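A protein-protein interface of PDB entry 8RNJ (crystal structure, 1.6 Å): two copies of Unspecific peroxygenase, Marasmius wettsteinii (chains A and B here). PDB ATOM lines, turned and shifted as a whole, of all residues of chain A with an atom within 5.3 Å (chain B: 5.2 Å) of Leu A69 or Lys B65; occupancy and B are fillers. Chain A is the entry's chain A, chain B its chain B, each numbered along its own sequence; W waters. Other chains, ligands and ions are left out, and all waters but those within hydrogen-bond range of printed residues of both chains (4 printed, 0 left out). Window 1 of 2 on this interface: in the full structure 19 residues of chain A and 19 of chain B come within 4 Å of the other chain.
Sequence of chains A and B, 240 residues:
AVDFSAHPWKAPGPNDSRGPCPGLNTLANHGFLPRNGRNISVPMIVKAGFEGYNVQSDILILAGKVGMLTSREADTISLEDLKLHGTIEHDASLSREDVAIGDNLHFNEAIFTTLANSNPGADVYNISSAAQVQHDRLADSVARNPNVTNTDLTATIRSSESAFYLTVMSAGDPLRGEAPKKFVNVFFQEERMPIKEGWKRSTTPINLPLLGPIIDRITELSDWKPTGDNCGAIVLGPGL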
ATOM      1  N   LYS A  65     -21.429  23.284 -21.365  1.00  0.00           N
ATOM      2  CA  LYS A  65     -21.020  22.076 -20.647  1.00  0.00           C
ATOM      3  C   LYS A  65     -19.492  21.962 -20.555  1.00  0.00           C
ATOM      4  O   LYS A  65     -18.989  21.472 -19.553  1.00  0.00           O
ATOM      5  CB  LYS A  65     -21.655  20.832 -21.278  1.00  0.00           C
ATOM      6  CG  LYS A  65     -23.163  20.788 -21.094  1.00  0.00           C
ATOM      7  CD  LYS A  65     -23.807  19.455 -21.433  1.00  0.00           C
ATOM      8  CE  LYS A  65     -23.655  19.079 -22.883  1.00  0.00           C
ATOM      9  NZ  LYS A  65     -24.473  17.889 -23.223  1.00  0.00           N
ATOM     10  N   VAL A  66     -18.746  22.489 -21.542  1.00  0.00           N
ATOM     11  CA  VAL A  66     -17.295  22.559 -21.416  1.00  0.00           C
ATOM     12  C   VAL A  66     -16.945  23.561 -20.309  1.00  0.00           C
ATOM     13  O   VAL A  66     -16.116  23.273 -19.459  1.00  0.00           O
ATOM     14  CB  VAL A  66     -16.588  22.869 -22.750  1.00  0.00           C
ATOM     15  CG1 VAL A  66     -15.094  23.052 -22.567  1.00  0.00           C
ATOM     16  CG2 VAL A  66     -16.865  21.766 -23.779  1.00  0.00           C
ATOM     17  N   GLY A  67     -17.649  24.707 -20.267  1.00  0.00           N
ATOM     18  CA  GLY A  67     -17.423  25.695 -19.224  1.00  0.00           C
ATOM     19  C   GLY A  67     -17.698  25.167 -17.812  1.00  0.00           C
ATOM     20  O   GLY A  67     -16.997  25.546 -16.873  1.00  0.00           O
ATOM     21  N   MET A  68     -18.683  24.265 -17.668  1.00  0.00           N
ATOM     22  CA  MET A  68     -19.033  23.714 -16.366  1.00  0.00           C
ATOM     23  C   MET A  68     -17.838  22.985 -15.748  1.00  0.00           C
ATOM     24  O   MET A  68     -17.732  22.884 -14.520  1.00  0.00           O
ATOM     25  CB  MET A  68     -20.218  22.748 -16.446  1.00  0.00           C
ATOM     26  CG  MET A  68     -21.561  23.359 -16.805  1.00  0.00           C
ATOM     27  SD  MET A  68     -22.204  24.560 -15.591  1.00  0.00           S
ATOM     28  CE  MET A  68     -22.057  26.093 -16.510  1.00  0.00           C
ATOM     29  N   LEU A  69     -16.915  22.467 -16.582  1.00  0.00           N
ATOM     30  CA  LEU A  69     -15.764  21.730 -16.061  1.00  0.00           C
ATOM     31  C   LEU A  69     -14.879  22.594 -15.159  1.00  0.00           C
ATOM     32  O   LEU A  69     -14.168  22.037 -14.326  1.00  0.00           O
ATOM     33  CB  LEU A  69     -14.919  21.181 -17.217  1.00  0.00           C
ATOM     34  CG  LEU A  69     -15.609  20.266 -18.216  1.00  0.00           C
ATOM     35  CD1 LEU A  69     -14.650  19.937 -19.339  1.00  0.00           C
ATOM     36  CD2 LEU A  69     -16.152  18.991 -17.569  1.00  0.00           C
ATOM     37  N   THR A  70     -14.931  23.928 -15.297  1.00  0.00           N
ATOM     38  CA  THR A  70     -14.006  24.823 -14.617  1.00  0.00           C
ATOM     39  C   THR A  70     -14.327  25.017 -13.127  1.00  0.00           C
ATOM     40  O   THR A  70     -13.482  25.549 -12.406  1.00  0.00           O
ATOM     41  CB  THR A  70     -13.920  26.193 -15.310  1.00  0.00           C
ATOM     42  OG1 THR A  70     -15.162  26.898 -15.209  1.00  0.00           O
ATOM     43  CG2 THR A  70     -13.560  26.078 -16.776  1.00  0.00           C
ATOM     44  N   SER A  71     -15.520  24.609 -12.671  1.00  0.00           N
ATOM     45  CA  SER A  71     -15.909  24.763 -11.273  1.00  0.00           C
ATOM     46  C   SER A  71     -15.788  23.454 -10.497  1.00  0.00           C
ATOM     47  O   SER A  71     -15.585  22.404 -11.091  1.00  0.00           O
ATOM     48  CB  SER A  71     -17.309  25.264 -11.166  1.00  0.00           C
ATOM     49  OG  SER A  71     -18.242  24.224 -11.319  1.00  0.00           O
ATOM     50  N   ARG A  72     -15.974  23.550  -9.171  1.00  0.00           N
ATOM     51  CA  ARG A  72     -16.016  22.394  -8.295  1.00  0.00           C
ATOM     52  C   ARG A  72     -17.451  21.966  -8.000  1.00  0.00           C
ATOM     53  O   ARG A  72     -17.646  21.046  -7.204  1.00  0.00           O
ATOM     54  CB  ARG A  72     -15.274  22.706  -6.989  1.00  0.00           C
ATOM     55  CG  ARG A  72     -13.764  22.760  -7.174  1.00  0.00           C
ATOM     56  CD  ARG A  72     -12.985  22.456  -5.900  1.00  0.00           C
ATOM     57  NE  ARG A  72     -11.569  22.301  -6.199  1.00  0.00           N
ATOM     58  CZ  ARG A  72     -10.739  23.298  -6.474  1.00  0.00           C
ATOM     59  NH1 ARG A  72     -11.153  24.553  -6.408  1.00  0.00           N
ATOM     60  NH2 ARG A  72      -9.482  23.036  -6.792  1.00  0.00           N
ATOM     61  N   GLU A  73     -18.439  22.637  -8.602  1.00  0.00           N
ATOM     62  CA  GLU A  73     -19.837  22.370  -8.309  1.00  0.00           C
ATOM     63  C   GLU A  73     -20.422  21.397  -9.333  1.00  0.00           C
ATOM     64  O   GLU A  73     -19.938  21.293 -10.458  1.00  0.00           O
ATOM     65  CB  GLU A  73     -20.651  23.671  -8.262  1.00  0.00           C
ATOM     66  CG  GLU A  73     -20.342  24.538  -7.053  1.00  0.00           C
ATOM     67  CD  GLU A  73     -19.022  25.279  -7.124  1.00  0.00           C
ATOM     68  OE1 GLU A  73     -18.820  26.042  -8.090  1.00  0.00           O
ATOM     69  OE2 GLU A  73     -18.197  25.095  -6.204  1.00  0.00           O
ATOM     70  N   ALA A  74     -21.526  20.751  -8.943  1.00  0.00           N
ATOM     71  CA  ALA A  74     -22.150  19.708  -9.733  1.00  0.00           C
ATOM     72  C   ALA A  74     -22.701  20.221 -11.066  1.00  0.00           C
ATOM     73  O   ALA A  74     -22.611  19.508 -12.051  1.00  0.00           O
ATOM     74  CB  ALA A  74     -23.230  19.042  -8.929  1.00  0.00           C
ATOM     75  N   ASP A  75     -23.355  21.398 -11.090  1.00  0.00           N
ATOM     76  CA  ASP A  75     -24.022  21.826 -12.318  1.00  0.00           C
ATOM     77  C   ASP A  75     -24.045  23.349 -12.483  1.00  0.00           C
ATOM     78  O   ASP A  75     -24.859  23.854 -13.262  1.00  0.00           O
ATOM     79  CB  ASP A  75     -25.436  21.251 -12.411  1.00  0.00           C
ATOM     80  CG  ASP A  75     -26.451  21.844 -11.442  1.00  0.00           C
ATOM     81  OD1 ASP A  75     -26.035  22.612 -10.552  1.00  0.00           O
ATOM     82  OD2 ASP A  75     -27.657  21.510 -11.579  1.00  0.00           O
ATOM     83  N   THR A  76     -23.157  24.067 -11.776  1.00  0.00           N
ATOM     84  CA  THR A  76     -23.052  25.519 -11.890  1.00  0.00           C
ATOM     85  C   THR A  76     -21.601  25.957 -11.868  1.00  0.00           C
ATOM     86  O   THR A  76     -20.723  25.212 -11.448  1.00  0.00           O
ATOM     87  CB  THR A  76     -23.784  26.277 -10.776  1.00  0.00           C
ATOM     88  OG1 THR A  76     -23.267  25.882  -9.507  1.00  0.00           O
ATOM     89  CG2 THR A  76     -25.284  26.093 -10.801  1.00  0.00           C
ATOM     90  N   LEU A  84     -10.004  29.444 -15.992  1.00  0.00           N
ATOM     91  CA  LEU A  84      -9.127  28.282 -15.843  1.00  0.00           C
ATOM     92  C   LEU A  84      -8.405  28.020 -17.161  1.00  0.00           C
ATOM     93  O   LEU A  84      -9.034  27.661 -18.153  1.00  0.00           O
ATOM     94  CB  LEU A  84      -9.939  27.043 -15.442  1.00  0.00           C
ATOM     95  CG  LEU A  84      -9.139  25.753 -15.241  1.00  0.00           C
ATOM     96  CD1 LEU A  84      -8.096  25.882 -14.141  1.00  0.00           C
ATOM     97  CD2 LEU A  84     -10.074  24.603 -14.931  1.00  0.00           C
ATOM     98  N   THR A  87      -8.950  25.047 -20.367  1.00  0.00           N
ATOM     99  CA  THR A  87     -10.264  24.465 -20.599  1.00  0.00           C
ATOM    100  C   THR A  87     -10.840  25.154 -21.838  1.00  0.00           C
ATOM    101  O   THR A  87     -10.707  24.626 -22.934  1.00  0.00           O
ATOM    102  CB  THR A  87     -11.180  24.496 -19.367  1.00  0.00           C
ATOM    103  OG1 THR A  87     -10.518  23.872 -18.263  1.00  0.00           O
ATOM    104  CG2 THR A  87     -12.504  23.813 -19.621  1.00  0.00           C
ATOM    105  N   ILE A 234      -7.965  19.324 -23.357  1.00  0.00           N
ATOM    106  CA  ILE A 234      -8.451  20.343 -22.428  1.00  0.00           C
ATOM    107  C   ILE A 234      -8.172  19.895 -20.997  1.00  0.00           C
ATOM    108  O   ILE A 234      -8.073  18.695 -20.704  1.00  0.00           O
ATOM    109  CB  ILE A 234      -9.948  20.669 -22.628  1.00  0.00           C
ATOM    110  CG1 ILE A 234     -10.866  19.464 -22.398  1.00  0.00           C
ATOM    111  CG2 ILE A 234     -10.196  21.294 -23.992  1.00  0.00           C
ATOM    112  CD1 ILE A 234     -12.278  19.851 -22.007  1.00  0.00           C
ATOM    113  N   VAL A 235      -8.095  20.879 -20.100  1.00  0.00           N
ATOM    114  CA  VAL A 235      -8.062  20.681 -18.660  1.00  0.00           C
ATOM    115  C   VAL A 235      -9.474  20.309 -18.209  1.00  0.00           C
ATOM    116  O   VAL A 235     -10.427  20.988 -18.573  1.00  0.00           O
ATOM    117  CB  VAL A 235      -7.537  21.958 -17.969  1.00  0.00           C
ATOM    118  CG1 VAL A 235      -7.705  21.929 -16.458  1.00  0.00           C
ATOM    119  CG2 VAL A 235      -6.088  22.230 -18.362  1.00  0.00           C
ATOM    120  N   LEU A 236      -9.614  19.204 -17.462  1.00  0.00           N
ATOM    121  CA  LEU A 236     -10.916  18.598 -17.193  1.00  0.00           C
ATOM    122  C   LEU A 236     -11.539  19.052 -15.875  1.00  0.00           C
ATOM    123  O   LEU A 236     -12.698  18.751 -15.612  1.00  0.00           O
ATOM    124  CB  LEU A 236     -10.764  17.077 -17.213  1.00  0.00           C
ATOM    125  CG  LEU A 236     -10.419  16.502 -18.588  1.00  0.00           C
ATOM    126  CD1 LEU A 236     -10.140  15.007 -18.517  1.00  0.00           C
ATOM    127  CD2 LEU A 236     -11.522  16.780 -19.592  1.00  0.00           C
ATOM    128  N   GLY A 237     -10.785  19.787 -15.065  1.00  0.00           N
ATOM    129  CA  GLY A 237     -11.288  20.281 -13.798  1.00  0.00           C
ATOM    130  C   GLY A 237     -10.258  21.174 -13.130  1.00  0.00           C
ATOM    131  O   GLY A 237      -9.081  21.157 -13.509  1.00  0.00           O
ATOM    132  N   PRO A 238     -10.669  21.998 -12.142  1.00  0.00           N
ATOM    133  CA  PRO A 238      -9.734  22.852 -11.412  1.00  0.00           C
ATOM    134  C   PRO A 238      -8.852  22.007 -10.482  1.00  0.00           C
ATOM    135  O   PRO A 238      -9.259  20.932 -10.050  1.00  0.00           O
ATOM    136  CB  PRO A 238     -10.666  23.793 -10.637  1.00  0.00           C
ATOM    137  CG  PRO A 238     -11.922  22.987 -10.424  1.00  0.00           C
ATOM    138  CD  PRO A 238     -12.054  22.159 -11.688  1.00  0.00           C
ATOM    139  N   VAL B  42     -26.008  15.512 -13.178  1.00  0.00           N
ATOM    140  CA  VAL B  42     -24.893  15.301 -12.270  1.00  0.00           C
ATOM    141  C   VAL B  42     -25.405  15.316 -10.831  1.00  0.00           C
ATOM    142  O   VAL B  42     -25.017  14.438 -10.057  1.00  0.00           O
ATOM    143  CB  VAL B  42     -23.735  16.281 -12.505  1.00  0.00           C
ATOM    144  CG1 VAL B  42     -22.623  16.129 -11.483  1.00  0.00           C
ATOM    145  CG2 VAL B  42     -23.168  16.119 -13.907  1.00  0.00           C
ATOM    146  N   LEU B  60     -17.562  12.321  -8.134  1.00  0.00           N
ATOM    147  CA  LEU B  60     -18.725  12.209  -9.011  1.00  0.00           C
ATOM    148  C   LEU B  60     -18.987  13.499  -9.783  1.00  0.00           C
ATOM    149  O   LEU B  60     -19.486  13.423 -10.902  1.00  0.00           O
ATOM    150  CB  LEU B  60     -19.944  11.798  -8.190  1.00  0.00           C
ATOM    151  CG  LEU B  60     -19.817  10.430  -7.524  1.00  0.00           C
ATOM    152  CD1 LEU B  60     -21.013  10.120  -6.648  1.00  0.00           C
ATOM    153  CD2 LEU B  60     -19.647   9.339  -8.564  1.00  0.00           C
ATOM    154  N   ILE B  61     -18.664  14.663  -9.203  1.00  0.00           N
ATOM    155  CA  ILE B  61     -18.801  15.935  -9.904  1.00  0.00           C
ATOM    156  C   ILE B  61     -17.791  15.989 -11.049  1.00  0.00           C
ATOM    157  O   ILE B  61     -18.141  16.339 -12.173  1.00  0.00           O
ATOM    158  CB  ILE B  61     -18.660  17.120  -8.922  1.00  0.00           C
ATOM    159  CG1 ILE B  61     -19.905  17.228  -8.040  1.00  0.00           C
ATOM    160  CG2 ILE B  61     -18.383  18.426  -9.668  1.00  0.00           C
ATOM    161  CD1 ILE B  61     -19.783  18.191  -6.878  1.00  0.00           C
ATOM    162  N   LEU B  62     -16.542  15.609 -10.767  1.00  0.00           N
ATOM    163  CA  LEU B  62     -15.497  15.655 -11.784  1.00  0.00           C
ATOM    164  C   LEU B  62     -15.830  14.726 -12.954  1.00  0.00           C
ATOM    165  O   LEU B  62     -15.863  15.145 -14.105  1.00  0.00           O
ATOM    166  CB  LEU B  62     -14.163  15.295 -11.125  1.00  0.00           C
ATOM    167  CG  LEU B  62     -12.923  15.353 -12.015  1.00  0.00           C
ATOM    168  CD1 LEU B  62     -12.665  16.778 -12.498  1.00  0.00           C
ATOM    169  CD2 LEU B  62     -11.702  14.838 -11.270  1.00  0.00           C
ATOM    170  N   ALA B  63     -16.112  13.454 -12.649  1.00  0.00           N
ATOM    171  CA  ALA B  63     -16.460  12.489 -13.671  1.00  0.00           C
ATOM    172  C   ALA B  63     -17.802  12.803 -14.331  1.00  0.00           C
ATOM    173  O   ALA B  63     -17.949  12.682 -15.544  1.00  0.00           O
ATOM    174  CB  ALA B  63     -16.453  11.109 -13.058  1.00  0.00           C
ATOM    175  N   GLY B  64     -18.797  13.173 -13.531  1.00  0.00           N
ATOM    176  CA  GLY B  64     -20.135  13.425 -14.039  1.00  0.00           C
ATOM    177  C   GLY B  64     -20.168  14.530 -15.094  1.00  0.00           C
ATOM    178  O   GLY B  64     -20.846  14.379 -16.107  1.00  0.00           O
ATOM    179  N   LYS B  65     -19.471  15.652 -14.852  1.00  0.00           N
ATOM    180  CA  LYS B  65     -19.510  16.762 -15.794  1.00  0.00           C
ATOM    181  C   LYS B  65     -18.804  16.413 -17.106  1.00  0.00           C
ATOM    182  O   LYS B  65     -19.233  16.866 -18.169  1.00  0.00           O
ATOM    183  CB  LYS B  65     -18.981  18.046 -15.157  1.00  0.00           C
ATOM    184  CG  LYS B  65     -19.869  18.583 -14.048  1.00  0.00           C
ATOM    185  CD  LYS B  65     -19.496  19.974 -13.594  1.00  0.00           C
ATOM    186  CE  LYS B  65     -18.115  20.037 -12.990  1.00  0.00           C
ATOM    187  NZ  LYS B  65     -17.900  21.327 -12.283  1.00  0.00           N
ATOM    188  N   VAL B  66     -17.782  15.550 -17.054  1.00  0.00           N
ATOM    189  CA  VAL B  66     -17.165  15.057 -18.281  1.00  0.00           C
ATOM    190  C   VAL B  66     -18.168  14.156 -19.003  1.00  0.00           C
ATOM    191  O   VAL B  66     -18.351  14.292 -20.203  1.00  0.00           O
ATOM    192  CB  VAL B  66     -15.818  14.362 -18.000  1.00  0.00           C
ATOM    193  CG1 VAL B  66     -15.255  13.691 -19.245  1.00  0.00           C
ATOM    194  CG2 VAL B  66     -14.804  15.319 -17.396  1.00  0.00           C
ATOM    195  N   GLY B  67     -18.885  13.293 -18.261  1.00  0.00           N
ATOM    196  CA  GLY B  67     -19.906  12.446 -18.853  1.00  0.00           C
ATOM    197  C   GLY B  67     -21.040  13.236 -19.528  1.00  0.00           C
ATOM    198  O   GLY B  67     -21.592  12.797 -20.531  1.00  0.00           O
ATOM    199  N   MET B  68     -21.387  14.419 -19.001  1.00  0.00           N
ATOM    200  CA  MET B  68     -22.463  15.226 -19.563  1.00  0.00           C
ATOM    201  C   MET B  68     -22.136  15.634 -21.002  1.00  0.00           C
ATOM    202  O   MET B  68     -23.038  15.854 -21.802  1.00  0.00           O
ATOM    203  CB  MET B  68     -22.705  16.493 -18.733  1.00  0.00           C
ATOM    204  CG  MET B  68     -23.317  16.252 -17.339  1.00  0.00           C
ATOM    205  SD  MET B  68     -24.975  15.527 -17.318  1.00  0.00           S
ATOM    206  CE  MET B  68     -24.597  13.920 -16.631  1.00  0.00           C
ATOM    207  N   LEU B  69     -20.842  15.701 -21.359  1.00  0.00           N
ATOM    208  CA  LEU B  69     -20.450  16.078 -22.719  1.00  0.00           C
ATOM    209  C   LEU B  69     -20.988  15.098 -23.764  1.00  0.00           C
ATOM    210  O   LEU B  69     -21.090  15.489 -24.931  1.00  0.00           O
ATOM    211  CB  LEU B  69     -18.925  16.187 -22.840  1.00  0.00           C
ATOM    212  CG  LEU B  69     -18.225  17.137 -21.872  1.00  0.00           C
ATOM    213  CD1 LEU B  69     -16.719  17.024 -22.001  1.00  0.00           C
ATOM    214  CD2 LEU B  69     -18.655  18.588 -22.081  1.00  0.00           C
HETATM  215  O   HOH W   1     -20.314  19.393 -18.240  1.00  0.00           O
HETATM  216  O   HOH W   2     -15.181  17.984 -14.439  1.00  0.00           O
HETATM  217  O   HOH W   3     -15.000  19.943 -12.480  1.00  0.00           O
HETATM  218  O   HOH W   4     -22.059  18.122 -25.580  1.00  0.00           O
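The backbone carbonyl oxygen (O) of Met B68 lies within hydrogen-bond range of the side-chain amino group (NZ) of Lys A65, at 2.9 Å. NZ of Lys B65 sits at hydrogen-bond distance from O of Met A68 (2.7 Å). The side-chain amino group (NZ) of Lys B65 lies within hydrogen-bond range of the backbone carbonyl oxygen (O) of Ser A71 (2.8 Å). The side-chain amino group (NZ) of Lys B65 lies within hydrogen-bond range of the backbone carbonyl oxygen (O) of Glu A73, at 2.7 Å.
The side-chain hydroxyl of Ser A71 sits at hydrogen-bond distance from the backbone NH of Glu A73 (3.2 Å). The backbone carbonyl oxygen of Thr A76 sits at hydrogen-bond distance from the side-chain hydroxyl of Ser A71 (2.7 Å).
Leu B69 touches Lys A65. CD2 of Leu B69 touches N of Val A66, 3.9 Å away. CD2 of Leu A69 touches C of Lys B65 (3.7 Å). Val B66 touches Leu A69. CD1 of Ile B61 touches O of Arg A72 (3.6 Å). O of Ala A74 touches CG1 of Val B42, 3.4 Å away. Ile B61 touches Ala A74 (CD1 to N, 3.7 Å). CD of Lys B65 touches O of Ala A74, at 3.5 Å. Leu B62 touches Leu A236 (CD1 to O, 3.7 Å). CA of Gly A237 touches CD1 of Leu B62, 3.98 Å away.
Of the 19 printed residues of chain A, 10 touch a printed residue of chain B. Hydrophobic or aromatic side chains of chain A that line the printed part of chain B: Leu A69 and Ala A74. Hydrophobic or aromatic side chains of chain B within 4 Å of the printed part of chain A: Val B42, Ile B61, Leu B62, Val B66 and Leu B69. Among the printed residues, 15 pairs touch across the chains. Among the printed residues, no Asp or Glu carboxylate lies within 4 Å of a Lys or Arg side-chain nitrogen of the other chain.
Water W1 lies within hydrogen-bond range of the backbone carbonyl oxygen of Lys B65 (2.7 Å) and the backbone carbonyl oxygen of Lys A65 (2.8 Å). Water W2 lies within hydrogen-bond range of the backbone carbonyl oxygen (O) of Leu A236 (2.9 Å) and the backbone carbonyl oxygen (O) of Leu B62 (2.9 Å). Water W4 bridges the backbone carbonyl oxygen of Leu B69 (2.9 Å) and the side-chain amino group of Lys A65 (3.4 Å). Water W3 lies within hydrogen-bond range of O of Ser A71 (2.9 Å), O of Leu A69 (2.9 Å) and NZ of Lys B65 (3.2 Å).
Lys A65 touches Met B68, and with the chains exchanged Met A68 touches Lys B65. Lys A65 touches Leu B69, and with the chains exchanged Leu A69 touches Lys B65. Val A66 touches Leu B69, and with the chains exchanged Leu A69 touches Val B66.
Of chain B, only Lys B65 (3.7 Å) and Val B66 (3.8 Å) come within 4 Å of Leu A69. Lys B65 touches just these residues of chain A: Met A68, Leu A69, Ser A71, Glu A73 and Ala A74. Printed residues of chain A within 4 Å of Met B68: Lys A65. Printed residues of chain B within 4 Å of Lys A65: Met B68 and Leu B69. Of the printed residues of chain B, Glu A73 touches Ile B61 (3.4 Å) and Lys B65 (2.7 Å). Of the printed residues of chain B, Leu A236 touches Leu B62 (3.7 Å). Printed residues of chain A within 4 Å of Val B66: Leu A69. Asp A75 touches none of the printed residues of chain B. The nearest residue of chain A that does not touch Lys B65 is Arg A72 (4.3 Å). The nearest printed residue of chain B that does not touch Leu A236 is Val B66 (4.2 Å).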
